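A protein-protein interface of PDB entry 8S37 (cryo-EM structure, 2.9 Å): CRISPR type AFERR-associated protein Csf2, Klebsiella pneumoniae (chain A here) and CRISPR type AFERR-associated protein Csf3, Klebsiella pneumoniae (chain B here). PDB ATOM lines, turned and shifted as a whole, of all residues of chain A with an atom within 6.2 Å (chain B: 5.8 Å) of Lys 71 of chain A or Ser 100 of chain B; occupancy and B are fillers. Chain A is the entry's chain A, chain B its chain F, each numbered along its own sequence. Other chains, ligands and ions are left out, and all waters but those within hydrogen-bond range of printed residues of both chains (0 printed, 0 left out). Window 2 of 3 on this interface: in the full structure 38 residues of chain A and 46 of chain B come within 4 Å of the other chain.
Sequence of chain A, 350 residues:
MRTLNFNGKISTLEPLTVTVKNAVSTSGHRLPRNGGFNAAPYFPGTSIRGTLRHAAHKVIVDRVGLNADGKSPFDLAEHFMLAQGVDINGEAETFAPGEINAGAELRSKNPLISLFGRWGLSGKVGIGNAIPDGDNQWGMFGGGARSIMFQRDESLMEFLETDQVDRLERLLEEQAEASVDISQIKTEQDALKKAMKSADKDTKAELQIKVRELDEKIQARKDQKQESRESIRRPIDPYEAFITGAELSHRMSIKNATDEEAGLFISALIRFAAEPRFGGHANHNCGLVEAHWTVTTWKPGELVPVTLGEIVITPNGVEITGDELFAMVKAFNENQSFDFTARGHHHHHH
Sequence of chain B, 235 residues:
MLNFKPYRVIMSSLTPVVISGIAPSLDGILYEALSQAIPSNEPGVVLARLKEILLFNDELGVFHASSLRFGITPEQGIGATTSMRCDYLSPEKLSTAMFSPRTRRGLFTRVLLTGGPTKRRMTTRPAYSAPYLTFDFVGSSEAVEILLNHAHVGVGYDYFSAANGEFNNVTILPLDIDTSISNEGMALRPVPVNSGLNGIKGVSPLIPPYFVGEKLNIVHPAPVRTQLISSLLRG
Printed residues of chain B within 4 Å of Phe 74 of chain A: Met 98 (3.3 Å), Phe 99 (3.2 Å) and Ser 100 (2.7 Å). Printed residues of chain B within 4 Å of Leu 76 of chain A: Phe 99. Printed residues of chain A within 4 Å of Met 98 of chain B: Ser 72 (3.4 Å) and Phe 74 (3.3 Å). Of the printed residues of chain A, Ser 100 of chain B touches Lys 71 (3.3 Å), Ser 72 (2.3 Å) and Phe 74 (2.7 Å). The nearest residue of chain B that does not touch Lys 71 of chain A is Thr 96 of chain B (5.4 Å). The nearest residue of chain A that does not touch Ser 100 of chain B is Asp 75 of chain A (4.1 Å). The nearest printed residue of chain A that does not touch Thr 96 of chain B is Leu 66 of chain A (5.2 Å).
Of the 12 printed residues of chain A, 4 touch a printed residue of chain B. Printed residues of chain A that touch a printed residue of chain B: Lys 71, Ser 72, Phe 74 and Leu 76. Hydrophobic or aromatic side chains of chain A that line the printed part of chain B: Phe 74 and Leu 76. Hydrophobic or aromatic side chains of chain B within 4 Å of the printed part of chain A: Phe 99. Among the printed residues, 9 pairs touch across the chains.
The backbone carbonyl oxygen (O) of Phe 74 of chain A sits at hydrogen-bond distance from the backbone NH (N) of Ser 100 of chain B, 2.7 Å away. The backbone carbonyl oxygen (O) of Thr 96 of chain B lies within hydrogen-bond range of the side-chain hydroxyl (OG) of Ser 72 of chain A (3.4 Å). The backbone NH (N) of Ser 72 of chain A lies within hydrogen-bond range of the side-chain hydroxyl (OG) of Ser 100 of chain B (3.3 Å).
Lys 71 of chain A touches Ser 100 of chain B (CB to OG, 3.3 Å). Ser 72 of chain A touches Met 98 of chain B (OG to C, 3.4 Å). Ser 72 of chain A touches Phe 99 of chain B. CD2 of Phe 74 of chain A touches O of Met 98 of chain B, 3.3 Å away. Phe 74 of chain A touches Phe 99 of chain B. Leu 76 of chain A touches Phe 99 of chain B (CD1 to CE2, 3.9 Å).
ND2 of Asn 67 of chain A sits at hydrogen-bond distance from O of Lys 71 of chain A, at 3.4 Å. NZ of Lys 71 of chain A lies within salt-bridge range of OD2 of Asp 69 of chain A, 3.5 Å away.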
ATOM      1  N   GLY A  65      -4.071  21.640  19.648  1.00  0.00           N
ATOM      2  CA  GLY A  65      -4.897  21.437  20.816  1.00  0.00           C
ATOM      3  C   GLY A  65      -4.128  20.741  21.923  1.00  0.00           C
ATOM      4  O   GLY A  65      -2.893  20.711  21.948  1.00  0.00           O
ATOM      5  N   LEU A  66      -4.884  20.168  22.853  1.00  0.00           N
ATOM      6  CA  LEU A  66      -4.334  19.464  24.000  1.00  0.00           C
ATOM      7  C   LEU A  66      -4.693  17.987  23.927  1.00  0.00           C
ATOM      8  O   LEU A  66      -5.687  17.599  23.307  1.00  0.00           O
ATOM      9  CB  LEU A  66      -4.860  20.055  25.310  1.00  0.00           C
ATOM     10  CG  LEU A  66      -4.519  21.523  25.567  1.00  0.00           C
ATOM     11  CD1 LEU A  66      -5.305  22.047  26.756  1.00  0.00           C
ATOM     12  CD2 LEU A  66      -3.027  21.695  25.795  1.00  0.00           C
ATOM     13  N   ASN A  67      -3.870  17.167  24.570  1.00  0.00           N
ATOM     14  CA  ASN A  67      -4.134  15.742  24.660  1.00  0.00           C
ATOM     15  C   ASN A  67      -5.376  15.493  25.512  1.00  0.00           C
ATOM     16  O   ASN A  67      -5.967  16.408  26.094  1.00  0.00           O
ATOM     17  CB  ASN A  67      -2.923  15.015  25.238  1.00  0.00           C
ATOM     18  CG  ASN A  67      -1.765  14.952  24.268  1.00  0.00           C
ATOM     19  OD1 ASN A  67      -1.959  14.902  23.054  1.00  0.00           O
ATOM     20  ND2 ASN A  67      -0.549  14.946  24.799  1.00  0.00           N
ATOM     21  N   ALA A  68      -5.775  14.221  25.585  1.00  0.00           N
ATOM     22  CA  ALA A  68      -6.877  13.836  26.459  1.00  0.00           C
ATOM     23  C   ALA A  68      -6.585  14.191  27.910  1.00  0.00           C
ATOM     24  O   ALA A  68      -7.515  14.413  28.695  1.00  0.00           O
ATOM     25  CB  ALA A  68      -7.154  12.339  26.324  1.00  0.00           C
ATOM     26  N   ASP A  69      -5.309  14.256  28.284  1.00  0.00           N
ATOM     27  CA  ASP A  69      -4.905  14.570  29.646  1.00  0.00           C
ATOM     28  C   ASP A  69      -4.846  16.067  29.916  1.00  0.00           C
ATOM     29  O   ASP A  69      -4.524  16.463  31.041  1.00  0.00           O
ATOM     30  CB  ASP A  69      -3.537  13.949  29.939  1.00  0.00           C
ATOM     31  CG  ASP A  69      -3.445  12.507  29.487  1.00  0.00           C
ATOM     32  OD1 ASP A  69      -4.494  11.832  29.435  1.00  0.00           O
ATOM     33  OD2 ASP A  69      -2.324  12.050  29.181  1.00  0.00           O
ATOM     34  N   GLY A  70      -5.139  16.905  28.924  1.00  0.00           N
ATOM     35  CA  GLY A  70      -5.080  18.337  29.123  1.00  0.00           C
ATOM     36  C   GLY A  70      -3.682  18.903  29.165  1.00  0.00           C
ATOM     37  O   GLY A  70      -3.467  19.959  29.768  1.00  0.00           O
ATOM     38  N   LYS A  71      -2.721  18.227  28.542  1.00  0.00           N
ATOM     39  CA  LYS A  71      -1.341  18.683  28.467  1.00  0.00           C
ATOM     40  C   LYS A  71      -0.932  18.792  27.007  1.00  0.00           C
ATOM     41  O   LYS A  71      -1.292  17.940  26.188  1.00  0.00           O
ATOM     42  CB  LYS A  71      -0.401  17.728  29.203  1.00  0.00           C
ATOM     43  CG  LYS A  71      -0.834  17.408  30.623  1.00  0.00           C
ATOM     44  CD  LYS A  71       0.285  16.761  31.435  1.00  0.00           C
ATOM     45  CE  LYS A  71       0.833  15.497  30.780  1.00  0.00           C
ATOM     46  NZ  LYS A  71      -0.238  14.532  30.412  1.00  0.00           N
ATOM     47  N   SER A  72      -0.201  19.854  26.687  1.00  0.00           N
ATOM     48  CA  SER A  72       0.250  20.064  25.320  1.00  0.00           C
ATOM     49  C   SER A  72       1.065  18.862  24.846  1.00  0.00           C
ATOM     50  O   SER A  72       1.894  18.343  25.603  1.00  0.00           O
ATOM     51  CB  SER A  72       1.091  21.335  25.227  1.00  0.00           C
ATOM     52  OG  SER A  72       0.298  22.487  25.444  1.00  0.00           O
ATOM     53  N   PRO A  73       0.865  18.384  23.612  1.00  0.00           N
ATOM     54  CA  PRO A  73       1.654  17.227  23.155  1.00  0.00           C
ATOM     55  C   PRO A  73       3.140  17.507  23.040  1.00  0.00           C
ATOM     56  O   PRO A  73       3.925  16.556  22.944  1.00  0.00           O
ATOM     57  CB  PRO A  73       1.051  16.901  21.781  1.00  0.00           C
ATOM     58  CG  PRO A  73      -0.264  17.557  21.761  1.00  0.00           C
ATOM     59  CD  PRO A  73      -0.135  18.776  22.601  1.00  0.00           C
ATOM     60  N   PHE A  74       3.554  18.770  23.049  1.00  0.00           N
ATOM     61  CA  PHE A  74       4.949  19.110  22.815  1.00  0.00           C
ATOM     62  C   PHE A  74       5.754  18.967  24.097  1.00  0.00           C
ATOM     63  O   PHE A  74       5.334  19.431  25.161  1.00  0.00           O
ATOM     64  CB  PHE A  74       5.066  20.535  22.283  1.00  0.00           C
ATOM     65  CG  PHE A  74       4.199  20.806  21.095  1.00  0.00           C
ATOM     66  CD1 PHE A  74       4.418  20.149  19.901  1.00  0.00           C
ATOM     67  CD2 PHE A  74       3.168  21.724  21.171  1.00  0.00           C
ATOM     68  CE1 PHE A  74       3.623  20.397  18.806  1.00  0.00           C
ATOM     69  CE2 PHE A  74       2.370  21.976  20.078  1.00  0.00           C
ATOM     70  CZ  PHE A  74       2.598  21.312  18.894  1.00  0.00           C
ATOM     71  N   ASP A  75       6.906  18.314  23.992  1.00  0.00           N
ATOM     72  CA  ASP A  75       7.852  18.237  25.092  1.00  0.00           C
ATOM     73  C   ASP A  75       8.829  19.405  24.987  1.00  0.00           C
ATOM     74  O   ASP A  75       8.694  20.283  24.132  1.00  0.00           O
ATOM     75  CB  ASP A  75       8.581  16.894  25.079  1.00  0.00           C
ATOM     76  CG  ASP A  75       9.345  16.654  23.791  1.00  0.00           C
ATOM     77  OD1 ASP A  75       9.175  17.445  22.839  1.00  0.00           O
ATOM     78  OD2 ASP A  75      10.116  15.675  23.730  1.00  0.00           O
ATOM     79  N   LEU A  76       9.829  19.423  25.869  1.00  0.00           N
ATOM     80  CA  LEU A  76      10.774  20.533  25.870  1.00  0.00           C
ATOM     81  C   LEU A  76      11.551  20.598  24.563  1.00  0.00           C
ATOM     82  O   LEU A  76      11.794  21.687  24.030  1.00  0.00           O
ATOM     83  CB  LEU A  76      11.727  20.406  27.056  1.00  0.00           C
ATOM     84  CG  LEU A  76      12.676  21.581  27.296  1.00  0.00           C
ATOM     85  CD1 LEU A  76      11.901  22.849  27.608  1.00  0.00           C
ATOM     86  CD2 LEU A  76      13.643  21.253  28.420  1.00  0.00           C
ATOM     87  N   THR B  96       2.848  25.801  30.698  1.00  0.00           N
ATOM     88  CA  THR B  96       2.323  24.495  30.328  1.00  0.00           C
ATOM     89  C   THR B  96       1.331  24.570  29.179  1.00  0.00           C
ATOM     90  O   THR B  96       1.020  23.536  28.580  1.00  0.00           O
ATOM     91  CB  THR B  96       1.655  23.836  31.532  1.00  0.00           C
ATOM     92  OG1 THR B  96       0.685  24.729  32.091  1.00  0.00           O
ATOM     93  CG2 THR B  96       2.684  23.486  32.587  1.00  0.00           C
ATOM     94  N   MET B  98       1.806  25.697  26.282  1.00  0.00           N
ATOM     95  CA  MET B  98       2.486  25.468  25.015  1.00  0.00           C
ATOM     96  C   MET B  98       3.251  24.157  24.949  1.00  0.00           C
ATOM     97  O   MET B  98       3.524  23.679  23.845  1.00  0.00           O
ATOM     98  CB  MET B  98       3.456  26.620  24.726  1.00  0.00           C
ATOM     99  CG  MET B  98       2.767  27.971  24.625  1.00  0.00           C
ATOM    100  SD  MET B  98       3.901  29.337  24.326  1.00  0.00           S
ATOM    101  CE  MET B  98       4.507  28.926  22.695  1.00  0.00           C
ATOM    102  N   PHE B  99       3.607  23.566  26.086  1.00  0.00           N
ATOM    103  CA  PHE B  99       4.346  22.312  26.089  1.00  0.00           C
ATOM    104  C   PHE B  99       4.154  21.643  27.441  1.00  0.00           C
ATOM    105  O   PHE B  99       3.637  22.246  28.382  1.00  0.00           O
ATOM    106  CB  PHE B  99       5.825  22.537  25.775  1.00  0.00           C
ATOM    107  CG  PHE B  99       6.612  23.095  26.915  1.00  0.00           C
ATOM    108  CD1 PHE B  99       6.561  24.442  27.212  1.00  0.00           C
ATOM    109  CD2 PHE B  99       7.419  22.274  27.678  1.00  0.00           C
ATOM    110  CE1 PHE B  99       7.292  24.958  28.257  1.00  0.00           C
ATOM    111  CE2 PHE B  99       8.153  22.785  28.721  1.00  0.00           C
ATOM    112  CZ  PHE B  99       8.089  24.128  29.012  1.00  0.00           C
ATOM    113  N   SER B 100       4.547  20.369  27.512  1.00  0.00           N
ATOM    114  CA  SER B 100       4.399  19.560  28.715  1.00  0.00           C
ATOM    115  C   SER B 100       5.756  19.394  29.395  1.00  0.00           C
ATOM    116  O   SER B 100       6.535  18.516  28.998  1.00  0.00           O
ATOM    117  CB  SER B 100       3.808  18.195  28.361  1.00  0.00           C
ATOM    118  OG  SER B 100       2.528  18.337  27.771  1.00  0.00           O
ATOM    119  N   PRO B 101       6.094  20.193  30.408  1.00  0.00           N
ATOM    120  CA  PRO B 101       7.371  19.989  31.100  1.00  0.00           C
ATOM    121  C   PRO B 101       7.404  18.654  31.821  1.00  0.00           C
ATOM    122  O   PRO B 101       6.383  18.158  32.305  1.00  0.00           O
ATOM    123  CB  PRO B 101       7.437  21.152  32.098  1.00  0.00           C
ATOM    124  CG  PRO B 101       6.353  22.079  31.722  1.00  0.00           C
ATOM    125  CD  PRO B 101       5.317  21.274  31.034  1.00  0.00           C
ATOM    126  N   ARG B 102       8.594  18.066  31.887  1.00  0.00           N
ATOM    127  CA  ARG B 102       8.761  16.851  32.668  1.00  0.00           C
ATOM    128  C   ARG B 102       8.522  17.159  34.140  1.00  0.00           C
ATOM    129  O   ARG B 102       9.126  18.075  34.704  1.00  0.00           O
ATOM    130  CB  ARG B 102      10.159  16.269  32.462  1.00  0.00           C
ATOM    131  CG  ARG B 102      10.449  15.881  31.023  1.00  0.00           C
ATOM    132  CD  ARG B 102      11.398  14.696  30.942  1.00  0.00           C
ATOM    133  NE  ARG B 102      12.652  14.935  31.648  1.00  0.00           N
ATOM    134  CZ  ARG B 102      13.681  15.615  31.156  1.00  0.00           C
ATOM    135  NH1 ARG B 102      13.635  16.176  29.958  1.00  0.00           N
ATOM    136  NH2 ARG B 102      14.784  15.736  31.887  1.00  0.00           N
